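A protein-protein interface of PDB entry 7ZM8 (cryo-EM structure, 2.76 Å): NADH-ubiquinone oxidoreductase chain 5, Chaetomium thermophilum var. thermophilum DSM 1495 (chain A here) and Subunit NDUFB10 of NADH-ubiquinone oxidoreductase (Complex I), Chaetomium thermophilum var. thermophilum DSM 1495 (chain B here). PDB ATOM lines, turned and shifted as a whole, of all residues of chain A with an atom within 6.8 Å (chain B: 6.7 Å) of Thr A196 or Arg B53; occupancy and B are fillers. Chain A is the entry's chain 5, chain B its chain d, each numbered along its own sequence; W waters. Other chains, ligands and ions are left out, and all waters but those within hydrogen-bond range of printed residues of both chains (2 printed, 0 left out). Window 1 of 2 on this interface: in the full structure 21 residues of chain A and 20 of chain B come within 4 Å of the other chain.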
ATOM      1  N   GLU A  68       0.251  14.392  34.358  1.00  0.00           N
ATOM      2  CA  GLU A  68      -0.670  14.371  33.230  1.00  0.00           C
ATOM      3  C   GLU A  68       0.097  14.665  31.951  1.00  0.00           C
ATOM      4  O   GLU A  68       0.744  15.712  31.839  1.00  0.00           O
ATOM      5  CB  GLU A  68      -1.785  15.394  33.421  1.00  0.00           C
ATOM      6  CG  GLU A  68      -2.553  15.644  32.144  1.00  0.00           C
ATOM      7  CD  GLU A  68      -3.314  16.944  32.145  1.00  0.00           C
ATOM      8  OE1 GLU A  68      -3.289  17.659  33.164  1.00  0.00           O
ATOM      9  OE2 GLU A  68      -3.920  17.265  31.112  1.00  0.00           O
ATOM     10  N   TRP A  69       0.059  13.726  31.009  1.00  0.00           N
ATOM     11  CA  TRP A  69       0.681  13.877  29.698  1.00  0.00           C
ATOM     12  C   TRP A  69       2.202  13.891  29.773  1.00  0.00           C
ATOM     13  O   TRP A  69       2.873  13.843  28.739  1.00  0.00           O
ATOM     14  CB  TRP A  69       0.195  15.155  29.005  1.00  0.00           C
ATOM     15  CG  TRP A  69      -1.152  15.047  28.388  1.00  0.00           C
ATOM     16  CD1 TRP A  69      -2.248  15.793  28.686  1.00  0.00           C
ATOM     17  CD2 TRP A  69      -1.549  14.143  27.362  1.00  0.00           C
ATOM     18  NE1 TRP A  69      -3.307  15.407  27.916  1.00  0.00           N
ATOM     19  CE2 TRP A  69      -2.903  14.394  27.089  1.00  0.00           C
ATOM     20  CE3 TRP A  69      -0.892  13.142  26.645  1.00  0.00           C
ATOM     21  CZ2 TRP A  69      -3.611  13.679  26.135  1.00  0.00           C
ATOM     22  CZ3 TRP A  69      -1.594  12.443  25.704  1.00  0.00           C
ATOM     23  CH2 TRP A  69      -2.938  12.712  25.453  1.00  0.00           C
ATOM     24  N   PHE A  70       2.763  13.929  30.974  1.00  0.00           N
ATOM     25  CA  PHE A  70       4.206  13.921  31.172  1.00  0.00           C
ATOM     26  C   PHE A  70       4.596  12.574  31.760  1.00  0.00           C
ATOM     27  O   PHE A  70       4.258  12.274  32.908  1.00  0.00           O
ATOM     28  CB  PHE A  70       4.672  15.049  32.097  1.00  0.00           C
ATOM     29  CG  PHE A  70       4.473  16.441  31.552  1.00  0.00           C
ATOM     30  CD1 PHE A  70       3.742  16.672  30.398  1.00  0.00           C
ATOM     31  CD2 PHE A  70       5.034  17.525  32.204  1.00  0.00           C
ATOM     32  CE1 PHE A  70       3.561  17.949  29.913  1.00  0.00           C
ATOM     33  CE2 PHE A  70       4.858  18.807  31.717  1.00  0.00           C
ATOM     34  CZ  PHE A  70       4.121  19.015  30.569  1.00  0.00           C
ATOM     35  N   ILE A  71       5.297  11.767  30.975  1.00  0.00           N
ATOM     36  CA  ILE A  71       5.865  10.510  31.439  1.00  0.00           C
ATOM     37  C   ILE A  71       7.277  10.429  30.869  1.00  0.00           C
ATOM     38  O   ILE A  71       7.471  10.134  29.687  1.00  0.00           O
ATOM     39  CB  ILE A  71       5.005   9.293  31.059  1.00  0.00           C
ATOM     40  CG1 ILE A  71       5.697   7.983  31.429  1.00  0.00           C
ATOM     41  CG2 ILE A  71       4.565   9.332  29.609  1.00  0.00           C
ATOM     42  CD1 ILE A  71       5.868   7.779  32.886  1.00  0.00           C
ATOM     43  N   LEU A 189       3.450  19.161  22.109  1.00  0.00           N
ATOM     44  CA  LEU A 189       3.216  17.718  21.824  1.00  0.00           C
ATOM     45  C   LEU A 189       2.848  16.915  23.058  1.00  0.00           C
ATOM     46  O   LEU A 189       2.486  15.781  22.893  1.00  0.00           O
ATOM     47  CB  LEU A 189       4.477  17.164  21.166  1.00  0.00           C
ATOM     48  CG  LEU A 189       4.831  17.738  19.799  1.00  0.00           C
ATOM     49  CD1 LEU A 189       6.082  17.069  19.264  1.00  0.00           C
ATOM     50  CD2 LEU A 189       3.673  17.562  18.833  1.00  0.00           C
ATOM     51  N   GLY A 190       3.029  17.463  24.246  1.00  0.00           N
ATOM     52  CA  GLY A 190       2.591  16.787  25.478  1.00  0.00           C
ATOM     53  C   GLY A 190       3.656  15.912  26.094  1.00  0.00           C
ATOM     54  O   GLY A 190       3.646  15.788  27.299  1.00  0.00           O
ATOM     55  N   ASN A 191       4.647  15.488  25.327  1.00  0.00           N
ATOM     56  CA  ASN A 191       5.753  14.699  25.910  1.00  0.00           C
ATOM     57  C   ASN A 191       7.022  15.010  25.141  1.00  0.00           C
ATOM     58  O   ASN A 191       6.921  15.257  23.939  1.00  0.00           O
ATOM     59  CB  ASN A 191       5.522  13.188  25.841  1.00  0.00           C
ATOM     60  CG  ASN A 191       5.993  12.451  27.076  1.00  0.00           C
ATOM     61  OD1 ASN A 191       6.035  13.013  28.165  1.00  0.00           O
ATOM     62  ND2 ASN A 191       6.331  11.187  26.916  1.00  0.00           N
ATOM     63  N   LEU A 192       8.155  15.026  25.831  1.00  0.00           N
ATOM     64  CA  LEU A 192       9.409  15.194  25.102  1.00  0.00           C
ATOM     65  C   LEU A 192      10.225  13.908  24.963  1.00  0.00           C
ATOM     66  O   LEU A 192      11.417  13.887  25.222  1.00  0.00           O
ATOM     67  CB  LEU A 192      10.199  16.322  25.762  1.00  0.00           C
ATOM     68  CG  LEU A 192      10.497  16.288  27.266  1.00  0.00           C
ATOM     69  CD1 LEU A 192      11.659  15.447  27.651  1.00  0.00           C
ATOM     70  CD2 LEU A 192      10.730  17.698  27.741  1.00  0.00           C
ATOM     71  N   ASP A 193       9.625  12.844  24.438  1.00  0.00           N
ATOM     72  CA  ASP A 193      10.373  11.663  24.027  1.00  0.00           C
ATOM     73  C   ASP A 193      10.748  11.782  22.558  1.00  0.00           C
ATOM     74  O   ASP A 193      10.031  12.401  21.772  1.00  0.00           O
ATOM     75  CB  ASP A 193       9.565  10.387  24.240  1.00  0.00           C
ATOM     76  CG  ASP A 193       9.155  10.186  25.678  1.00  0.00           C
ATOM     77  OD1 ASP A 193       9.715  10.864  26.564  1.00  0.00           O
ATOM     78  OD2 ASP A 193       8.267   9.344  25.924  1.00  0.00           O
ATOM     79  N   TYR A 194      11.881  11.182  22.191  1.00  0.00           N
ATOM     80  CA  TYR A 194      12.388  11.346  20.830  1.00  0.00           C
ATOM     81  C   TYR A 194      11.436  10.754  19.806  1.00  0.00           C
ATOM     82  O   TYR A 194      11.163  11.372  18.771  1.00  0.00           O
ATOM     83  CB  TYR A 194      13.766  10.707  20.686  1.00  0.00           C
ATOM     84  CG  TYR A 194      14.857  11.411  21.445  1.00  0.00           C
ATOM     85  CD1 TYR A 194      14.755  12.753  21.751  1.00  0.00           C
ATOM     86  CD2 TYR A 194      15.988  10.735  21.849  1.00  0.00           C
ATOM     87  CE1 TYR A 194      15.744  13.398  22.436  1.00  0.00           C
ATOM     88  CE2 TYR A 194      16.983  11.376  22.532  1.00  0.00           C
ATOM     89  CZ  TYR A 194      16.856  12.707  22.824  1.00  0.00           C
ATOM     90  OH  TYR A 194      17.854  13.349  23.507  1.00  0.00           O
ATOM     91  N   ALA A 195      10.924   9.554  20.070  1.00  0.00           N
ATOM     92  CA  ALA A 195      10.008   8.929  19.129  1.00  0.00           C
ATOM     93  C   ALA A 195       8.759   9.774  18.950  1.00  0.00           C
ATOM     94  O   ALA A 195       8.237   9.896  17.837  1.00  0.00           O
ATOM     95  CB  ALA A 195       9.651   7.525  19.601  1.00  0.00           C
ATOM     96  N   THR A 196       8.267  10.370  20.034  1.00  0.00           N
ATOM     97  CA  THR A 196       7.086  11.219  19.953  1.00  0.00           C
ATOM     98  C   THR A 196       7.372  12.479  19.149  1.00  0.00           C
ATOM     99  O   THR A 196       6.609  12.839  18.248  1.00  0.00           O
ATOM    100  CB  THR A 196       6.615  11.584  21.359  1.00  0.00           C
ATOM    101  OG1 THR A 196       6.409  10.392  22.123  1.00  0.00           O
ATOM    102  CG2 THR A 196       5.315  12.360  21.298  1.00  0.00           C
ATOM    103  N   VAL A 197       8.474  13.157  19.460  1.00  0.00           N
ATOM    104  CA  VAL A 197       8.737  14.464  18.872  1.00  0.00           C
ATOM    105  C   VAL A 197       9.000  14.340  17.381  1.00  0.00           C
ATOM    106  O   VAL A 197       8.619  15.213  16.595  1.00  0.00           O
ATOM    107  CB  VAL A 197       9.900  15.152  19.611  1.00  0.00           C
ATOM    108  CG1 VAL A 197      10.280  16.449  18.935  1.00  0.00           C
ATOM    109  CG2 VAL A 197       9.514  15.417  21.051  1.00  0.00           C
ATOM    110  N   PHE A 198       9.627  13.232  16.986  1.00  0.00           N
ATOM    111  CA  PHE A 198      10.045  13.076  15.572  1.00  0.00           C
ATOM    112  C   PHE A 198       8.905  12.488  14.736  1.00  0.00           C
ATOM    113  O   PHE A 198       8.761  12.883  13.573  1.00  0.00           O
ATOM    114  CB  PHE A 198      11.364  12.305  15.518  1.00  0.00           C
ATOM    115  CG  PHE A 198      12.478  12.903  16.339  1.00  0.00           C
ATOM    116  CD1 PHE A 198      12.536  14.266  16.581  1.00  0.00           C
ATOM    117  CD2 PHE A 198      13.485  12.103  16.854  1.00  0.00           C
ATOM    118  CE1 PHE A 198      13.556  14.812  17.342  1.00  0.00           C
ATOM    119  CE2 PHE A 198      14.507  12.650  17.613  1.00  0.00           C
ATOM    120  CZ  PHE A 198      14.540  14.002  17.855  1.00  0.00           C
ATOM    121  N   SER A 199       8.099  11.606  15.321  1.00  0.00           N
ATOM    122  CA  SER A 199       6.958  11.071  14.591  1.00  0.00           C
ATOM    123  C   SER A 199       5.970  12.171  14.231  1.00  0.00           C
ATOM    124  O   SER A 199       5.405  12.170  13.134  1.00  0.00           O
ATOM    125  CB  SER A 199       6.280   9.981  15.415  1.00  0.00           C
ATOM    126  OG  SER A 199       5.970  10.454  16.707  1.00  0.00           O
ATOM    127  N   LEU A 200       5.760  13.122  15.134  1.00  0.00           N
ATOM    128  CA  LEU A 200       4.788  14.184  14.941  1.00  0.00           C
ATOM    129  C   LEU A 200       5.363  15.440  14.310  1.00  0.00           C
ATOM    130  O   LEU A 200       4.596  16.346  13.980  1.00  0.00           O
ATOM    131  CB  LEU A 200       4.153  14.553  16.280  1.00  0.00           C
ATOM    132  CG  LEU A 200       3.212  13.532  16.901  1.00  0.00           C
ATOM    133  CD1 LEU A 200       2.722  14.069  18.208  1.00  0.00           C
ATOM    134  CD2 LEU A 200       2.058  13.249  15.979  1.00  0.00           C
ATOM    135  N   ALA A 201       6.681  15.513  14.135  1.00  0.00           N
ATOM    136  CA  ALA A 201       7.308  16.744  13.656  1.00  0.00           C
ATOM    137  C   ALA A 201       6.786  17.248  12.314  1.00  0.00           C
ATOM    138  O   ALA A 201       6.607  18.471  12.180  1.00  0.00           O
ATOM    139  CB  ALA A 201       8.825  16.556  13.603  1.00  0.00           C
ATOM    140  N   ILE A 204       3.481  19.550  12.979  1.00  0.00           N
ATOM    141  CA  ILE A 204       3.395  20.647  13.936  1.00  0.00           C
ATOM    142  C   ILE A 204       3.388  21.991  13.214  1.00  0.00           C
ATOM    143  O   ILE A 204       3.940  22.147  12.121  1.00  0.00           O
ATOM    144  CB  ILE A 204       4.565  20.570  14.928  1.00  0.00           C
ATOM    145  CG1 ILE A 204       4.726  19.146  15.449  1.00  0.00           C
ATOM    146  CG2 ILE A 204       4.372  21.528  16.086  1.00  0.00           C
ATOM    147  CD1 ILE A 204       5.980  18.949  16.267  1.00  0.00           C
ATOM    148  N   VAL B  46      -6.595  10.631  29.582  1.00  0.00           N
ATOM    149  CA  VAL B  46      -5.168  11.026  29.455  1.00  0.00           C
ATOM    150  C   VAL B  46      -4.298   9.769  29.486  1.00  0.00           C
ATOM    151  O   VAL B  46      -3.252   9.764  28.821  1.00  0.00           O
ATOM    152  CB  VAL B  46      -4.761  12.110  30.474  1.00  0.00           C
ATOM    153  CG1 VAL B  46      -3.278  12.432  30.416  1.00  0.00           C
ATOM    154  CG2 VAL B  46      -5.587  13.375  30.316  1.00  0.00           C
ATOM    155  N   MET B  48      -5.371   7.004  28.193  1.00  0.00           N
ATOM    156  CA  MET B  48      -5.612   6.471  26.860  1.00  0.00           C
ATOM    157  C   MET B  48      -4.591   7.006  25.871  1.00  0.00           C
ATOM    158  O   MET B  48      -4.078   6.261  25.032  1.00  0.00           O
ATOM    159  CB  MET B  48      -7.024   6.826  26.402  1.00  0.00           C
ATOM    160  CG  MET B  48      -8.036   5.735  26.603  1.00  0.00           C
ATOM    161  SD  MET B  48      -9.705   6.338  26.413  1.00  0.00           S
ATOM    162  CE  MET B  48      -9.902   6.163  24.642  1.00  0.00           C
ATOM    163  N   GLY B  49      -4.295   8.305  25.952  1.00  0.00           N
ATOM    164  CA  GLY B  49      -3.263   8.884  25.108  1.00  0.00           C
ATOM    165  C   GLY B  49      -1.874   8.399  25.466  1.00  0.00           C
ATOM    166  O   GLY B  49      -1.042   8.175  24.587  1.00  0.00           O
ATOM    167  N   ARG B  50      -1.586   8.238  26.752  1.00  0.00           N
ATOM    168  CA  ARG B  50      -0.286   7.665  27.198  1.00  0.00           C
ATOM    169  C   ARG B  50      -0.019   6.330  26.497  1.00  0.00           C
ATOM    170  O   ARG B  50       1.084   6.174  25.968  1.00  0.00           O
ATOM    171  CB  ARG B  50      -0.241   7.572  28.725  1.00  0.00           C
ATOM    172  CG  ARG B  50       0.983   6.866  29.284  1.00  0.00           C
ATOM    173  CD  ARG B  50       1.000   6.891  30.798  1.00  0.00           C
ATOM    174  NE  ARG B  50       1.308   8.212  31.319  1.00  0.00           N
ATOM    175  CZ  ARG B  50       1.493   8.487  32.602  1.00  0.00           C
ATOM    176  NH1 ARG B  50       1.779   9.718  32.981  1.00  0.00           N
ATOM    177  NH2 ARG B  50       1.390   7.527  33.501  1.00  0.00           N
ATOM    178  N   LEU B  51      -0.976   5.396  26.537  1.00  0.00           N
ATOM    179  CA  LEU B  51      -0.851   4.049  25.928  1.00  0.00           C
ATOM    180  C   LEU B  51      -0.711   4.115  24.415  1.00  0.00           C
ATOM    181  O   LEU B  51       0.096   3.351  23.884  1.00  0.00           O
ATOM    182  CB  LEU B  51      -2.083   3.245  26.342  1.00  0.00           C
ATOM    183  CG  LEU B  51      -2.128   2.795  27.798  1.00  0.00           C
ATOM    184  CD1 LEU B  51      -3.392   2.002  28.068  1.00  0.00           C
ATOM    185  CD2 LEU B  51      -0.902   1.969  28.140  1.00  0.00           C
ATOM    186  N   VAL B  52      -1.466   4.984  23.746  1.00  0.00           N
ATOM    187  CA  VAL B  52      -1.312   5.178  22.269  1.00  0.00           C
ATOM    188  C   VAL B  52       0.107   5.685  21.986  1.00  0.00           C
ATOM    189  O   VAL B  52       0.707   5.196  21.034  1.00  0.00           O
ATOM    190  CB  VAL B  52      -2.401   6.099  21.682  1.00  0.00           C
ATOM    191  CG1 VAL B  52      -2.097   6.517  20.254  1.00  0.00           C
ATOM    192  CG2 VAL B  52      -3.778   5.469  21.760  1.00  0.00           C
ATOM    193  N   ARG B  53       0.637   6.586  22.813  1.00  0.00           N
ATOM    194  CA  ARG B  53       2.007   7.146  22.654  1.00  0.00           C
ATOM    195  C   ARG B  53       3.059   6.045  22.814  1.00  0.00           C
ATOM    196  O   ARG B  53       4.072   6.110  22.102  1.00  0.00           O
ATOM    197  CB  ARG B  53       2.191   8.370  23.555  1.00  0.00           C
ATOM    198  CG  ARG B  53       3.499   9.111  23.346  1.00  0.00           C
ATOM    199  CD  ARG B  53       4.073   9.594  24.656  1.00  0.00           C
ATOM    200  NE  ARG B  53       3.389  10.780  25.147  1.00  0.00           N
ATOM    201  CZ  ARG B  53       2.714  10.849  26.284  1.00  0.00           C
ATOM    202  NH1 ARG B  53       2.134  11.980  26.639  1.00  0.00           N
ATOM    203  NH2 ARG B  53       2.631   9.791  27.065  1.00  0.00           N
ATOM    204  N   GLU B  54       2.860   5.102  23.729  1.00  0.00           N
ATOM    205  CA  GLU B  54       3.777   3.941  23.870  1.00  0.00           C
ATOM    206  C   GLU B  54       3.764   3.070  22.608  1.00  0.00           C
ATOM    207  O   GLU B  54       4.831   2.605  22.213  1.00  0.00           O
ATOM    208  CB  GLU B  54       3.392   3.105  25.085  1.00  0.00           C
ATOM    209  CG  GLU B  54       3.335   3.887  26.380  1.00  0.00           C
ATOM    210  CD  GLU B  54       2.764   3.114  27.557  1.00  0.00           C
ATOM    211  OE1 GLU B  54       2.542   3.729  28.618  1.00  0.00           O
ATOM    212  OE2 GLU B  54       2.545   1.897  27.411  1.00  0.00           O
ATOM    213  N   GLU B  55       2.597   2.831  22.016  1.00  0.00           N
ATOM    214  CA  GLU B  55       2.520   2.062  20.747  1.00  0.00           C
ATOM    215  C   GLU B  55       3.190   2.848  19.615  1.00  0.00           C
ATOM    216  O   GLU B  55       3.897   2.230  18.812  1.00  0.00           O
ATOM    217  CB  GLU B  55       1.078   1.655  20.449  1.00  0.00           C
ATOM    218  CG  GLU B  55       0.444   0.805  21.526  1.00  0.00           C
ATOM    219  CD  GLU B  55       0.726  -0.682  21.410  1.00  0.00           C
ATOM    220  OE1 GLU B  55       0.504  -1.404  22.402  1.00  0.00           O
ATOM    221  OE2 GLU B  55       1.156  -1.118  20.325  1.00  0.00           O
ATOM    222  N   LEU B  56       2.969   4.159  19.561  1.00  0.00           N
ATOM    223  CA  LEU B  56       3.577   4.994  18.501  1.00  0.00           C
ATOM    224  C   LEU B  56       5.084   4.813  18.546  1.00  0.00           C
ATOM    225  O   LEU B  56       5.668   4.613  17.490  1.00  0.00           O
ATOM    226  CB  LEU B  56       3.179   6.459  18.699  1.00  0.00           C
ATOM    227  CG  LEU B  56       3.492   7.404  17.540  1.00  0.00           C
ATOM    228  CD1 LEU B  56       3.077   6.797  16.213  1.00  0.00           C
ATOM    229  CD2 LEU B  56       2.814   8.748  17.743  1.00  0.00           C
ATOM    230  N   SER B  57       5.663   4.877  19.747  1.00  0.00           N
ATOM    231  CA  SER B  57       7.131   4.747  19.922  1.00  0.00           C
ATOM    232  C   SER B  57       7.635   3.406  19.400  1.00  0.00           C
ATOM    233  O   SER B  57       8.726   3.382  18.817  1.00  0.00           O
ATOM    234  CB  SER B  57       7.528   4.983  21.343  1.00  0.00           C
ATOM    235  OG  SER B  57       7.181   3.877  22.160  1.00  0.00           O
ATOM    236  N   LYS B  58       6.864   2.339  19.586  1.00  0.00           N
ATOM    237  CA  LYS B  58       7.352   1.002  19.178  1.00  0.00           C
ATOM    238  C   LYS B  58       7.190   0.922  17.663  1.00  0.00           C
ATOM    239  O   LYS B  58       8.070   0.331  17.041  1.00  0.00           O
ATOM    240  CB  LYS B  58       6.613  -0.091  19.950  1.00  0.00           C
ATOM    241  CG  LYS B  58       6.861  -0.111  21.450  1.00  0.00           C
ATOM    242  CD  LYS B  58       6.010  -1.128  22.171  1.00  0.00           C
ATOM    243  CE  LYS B  58       4.529  -0.911  21.950  1.00  0.00           C
ATOM    244  NZ  LYS B  58       3.708  -1.844  22.755  1.00  0.00           N
ATOM    245  N   TYR B  60       7.573   3.490  15.792  1.00  0.00           N
ATOM    246  CA  TYR B  60       8.668   4.376  15.317  1.00  0.00           C
ATOM    247  C   TYR B  60       9.987   3.601  15.279  1.00  0.00           C
ATOM    248  O   TYR B  60      10.706   3.698  14.275  1.00  0.00           O
ATOM    249  CB  TYR B  60       8.811   5.595  16.228  1.00  0.00           C
ATOM    250  CG  TYR B  60       9.857   6.591  15.796  1.00  0.00           C
ATOM    251  CD1 TYR B  60      11.164   6.502  16.247  1.00  0.00           C
ATOM    252  CD2 TYR B  60       9.539   7.626  14.935  1.00  0.00           C
ATOM    253  CE1 TYR B  60      12.130   7.410  15.848  1.00  0.00           C
ATOM    254  CE2 TYR B  60      10.490   8.544  14.530  1.00  0.00           C
ATOM    255  CZ  TYR B  60      11.790   8.435  14.986  1.00  0.00           C
ATOM    256  OH  TYR B  60      12.729   9.339  14.587  1.00  0.00           O
ATOM    257  N   TYR B  61      10.309   2.867  16.345  1.00  0.00           N
ATOM    258  CA  TYR B  61      11.597   2.129  16.426  1.00  0.00           C
ATOM    259  C   TYR B  61      11.529   0.844  15.600  1.00  0.00           C
ATOM    260  O   TYR B  61      12.593   0.248  15.358  1.00  0.00           O
ATOM    261  CB  TYR B  61      12.009   1.949  17.889  1.00  0.00           C
ATOM    262  CG  TYR B  61      12.419   3.234  18.561  1.00  0.00           C
ATOM    263  CD1 TYR B  61      13.469   3.988  18.069  1.00  0.00           C
ATOM    264  CD2 TYR B  61      11.755   3.705  19.679  1.00  0.00           C
ATOM    265  CE1 TYR B  61      13.848   5.177  18.666  1.00  0.00           C
ATOM    266  CE2 TYR B  61      12.122   4.890  20.292  1.00  0.00           C
ATOM    267  CZ  TYR B  61      13.173   5.630  19.784  1.00  0.00           C
ATOM    268  OH  TYR B  61      13.545   6.799  20.382  1.00  0.00           O
ATOM    269  N   LEU B  74      -1.784   5.623  14.384  1.00  0.00           N
ATOM    270  CA  LEU B  74      -1.436   5.945  15.762  1.00  0.00           C
ATOM    271  C   LEU B  74      -1.200   7.438  15.934  1.00  0.00           C
ATOM    272  O   LEU B  74      -1.541   8.009  16.975  1.00  0.00           O
ATOM    273  CB  LEU B  74      -0.202   5.154  16.189  1.00  0.00           C
ATOM    274  CG  LEU B  74      -0.409   3.709  16.639  1.00  0.00           C
ATOM    275  CD1 LEU B  74       0.924   3.017  16.801  1.00  0.00           C
ATOM    276  CD2 LEU B  74      -1.191   3.658  17.936  1.00  0.00           C
ATOM    277  N   TYR B  78      -3.291   9.834  18.660  1.00  0.00           N
ATOM    278  CA  TYR B  78      -2.593  10.611  19.676  1.00  0.00           C
ATOM    279  C   TYR B  78      -2.864  12.101  19.522  1.00  0.00           C
ATOM    280  O   TYR B  78      -2.982  12.823  20.517  1.00  0.00           O
ATOM    281  CB  TYR B  78      -1.093  10.333  19.621  1.00  0.00           C
ATOM    282  CG  TYR B  78      -0.328  11.169  20.610  1.00  0.00           C
ATOM    283  CD1 TYR B  78      -0.394  10.903  21.970  1.00  0.00           C
ATOM    284  CD2 TYR B  78       0.422  12.251  20.190  1.00  0.00           C
ATOM    285  CE1 TYR B  78       0.283  11.679  22.878  1.00  0.00           C
ATOM    286  CE2 TYR B  78       1.099  13.032  21.091  1.00  0.00           C
ATOM    287  CZ  TYR B  78       1.028  12.742  22.433  1.00  0.00           C
ATOM    288  OH  TYR B  78       1.713  13.518  23.330  1.00  0.00           O
ATOM    289  N   LEU B  82      -4.641  14.418  22.235  1.00  0.00           N
ATOM    290  CA  LEU B  82      -3.860  15.534  22.755  1.00  0.00           C
ATOM    291  C   LEU B  82      -4.653  16.832  22.759  1.00  0.00           C
ATOM    292  O   LEU B  82      -4.451  17.682  23.632  1.00  0.00           O
ATOM    293  CB  LEU B  82      -2.584  15.698  21.935  1.00  0.00           C
ATOM    294  CG  LEU B  82      -1.531  16.649  22.495  1.00  0.00           C
ATOM    295  CD1 LEU B  82      -1.123  16.239  23.896  1.00  0.00           C
ATOM    296  CD2 LEU B  82      -0.345  16.686  21.567  1.00  0.00           C
HETATM  297  O   HOH W   1       5.538   8.274  20.402  1.00  0.00           O
HETATM  298  O   HOH W   2      -4.043  17.861  26.133  1.00  0.00           O
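NH1 of Arg B53 is in hydrogen-bond range of O of Trp A69. NE of Arg B53 sits close to ND2 of Asn A191, 3.5 Å away. OH of Tyr B78 is in hydrogen-bond range of O of Leu A189 (2.4 Å).
The backbone carbonyl oxygen (O) of Glu B54 sits at hydrogen-bond distance from the side-chain hydroxyl (OG) of Ser B57 (2.7 Å). The backbone carbonyl oxygen of Trp A69 sits close to the backbone carbonyl oxygen of Gly A190. N of Ile A71 sits at hydrogen-bond distance from OD1 of Asn A191 (3.2 Å). The side-chain carboxylate of Asp A193 sits at hydrogen-bond distance from the side-chain amide nitrogen of Asn A191, 2.9 Å away. O of Ala A195 sits at hydrogen-bond distance from OG of Ser A199 (2.6 Å). O of Thr A196 lies within hydrogen-bond range of OG of Ser A199.
Among the printed residues, pairs that only touch across the chains: Glu A68 with Val B46, Trp A69 with Val B46, Trp A69 with Gly B49, Trp A69 with Tyr B78, Trp A69 with Leu B82, Phe A70 with Arg B50, Ile A71 with Arg B50, Ile A71 with Arg B53, Leu A189 with Leu B82, Tyr A194 with Tyr B61, Ala A195 with Ser B57, Ala A195 with Tyr B60, Ala A195 with Tyr B61, Thr A196 with Arg B53, Phe A198 with Tyr B60, Ser A199 with Leu B56, Ser A199 with Tyr B60 and Leu A200 with Tyr B78.
Of the printed residues of chain B, Tyr A194 touches Tyr B61 (3.9 Å). Of the printed residues of chain B, Ser A199 touches Leu B56 (3.7 Å) and Tyr B60 (3.96 Å). Leu B51 touches none of the printed residues of chain A. Of chain A, only Trp A69 (2.9 Å), Ile A71 (3.2 Å), Asn A191 (3.3 Å) and Thr A196 (3.4 Å) come within 4 Å of Arg B53. Of the printed residues of chain A, Leu B56 touches Ser A199. Printed residues of chain A within 4 Å of Ser B57: Ala A195 (3.7 Å). The nearest residue of chain A that does not touch Arg B53 is Gly A190 (4.2 Å).
Printed residues of chain A that touch a printed residue of chain B: Glu A68, Trp A69, Phe A70, Ile A71, Leu A189, Asn A191, Tyr A194, Ala A195, Thr A196, Phe A198, Ser A199 and Leu A200.
Water W2 bridges O of Leu B82 (2.5 Å) and NE1 of Trp A69 (3.1 Å). Water W1 lies within hydrogen-bond range of the side-chain hydroxyl of Thr A196 (2.9 Å), the backbone carbonyl oxygen of Arg B53 (3.1 Å) and the backbone NH of Ser B57 (3.5 Å).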
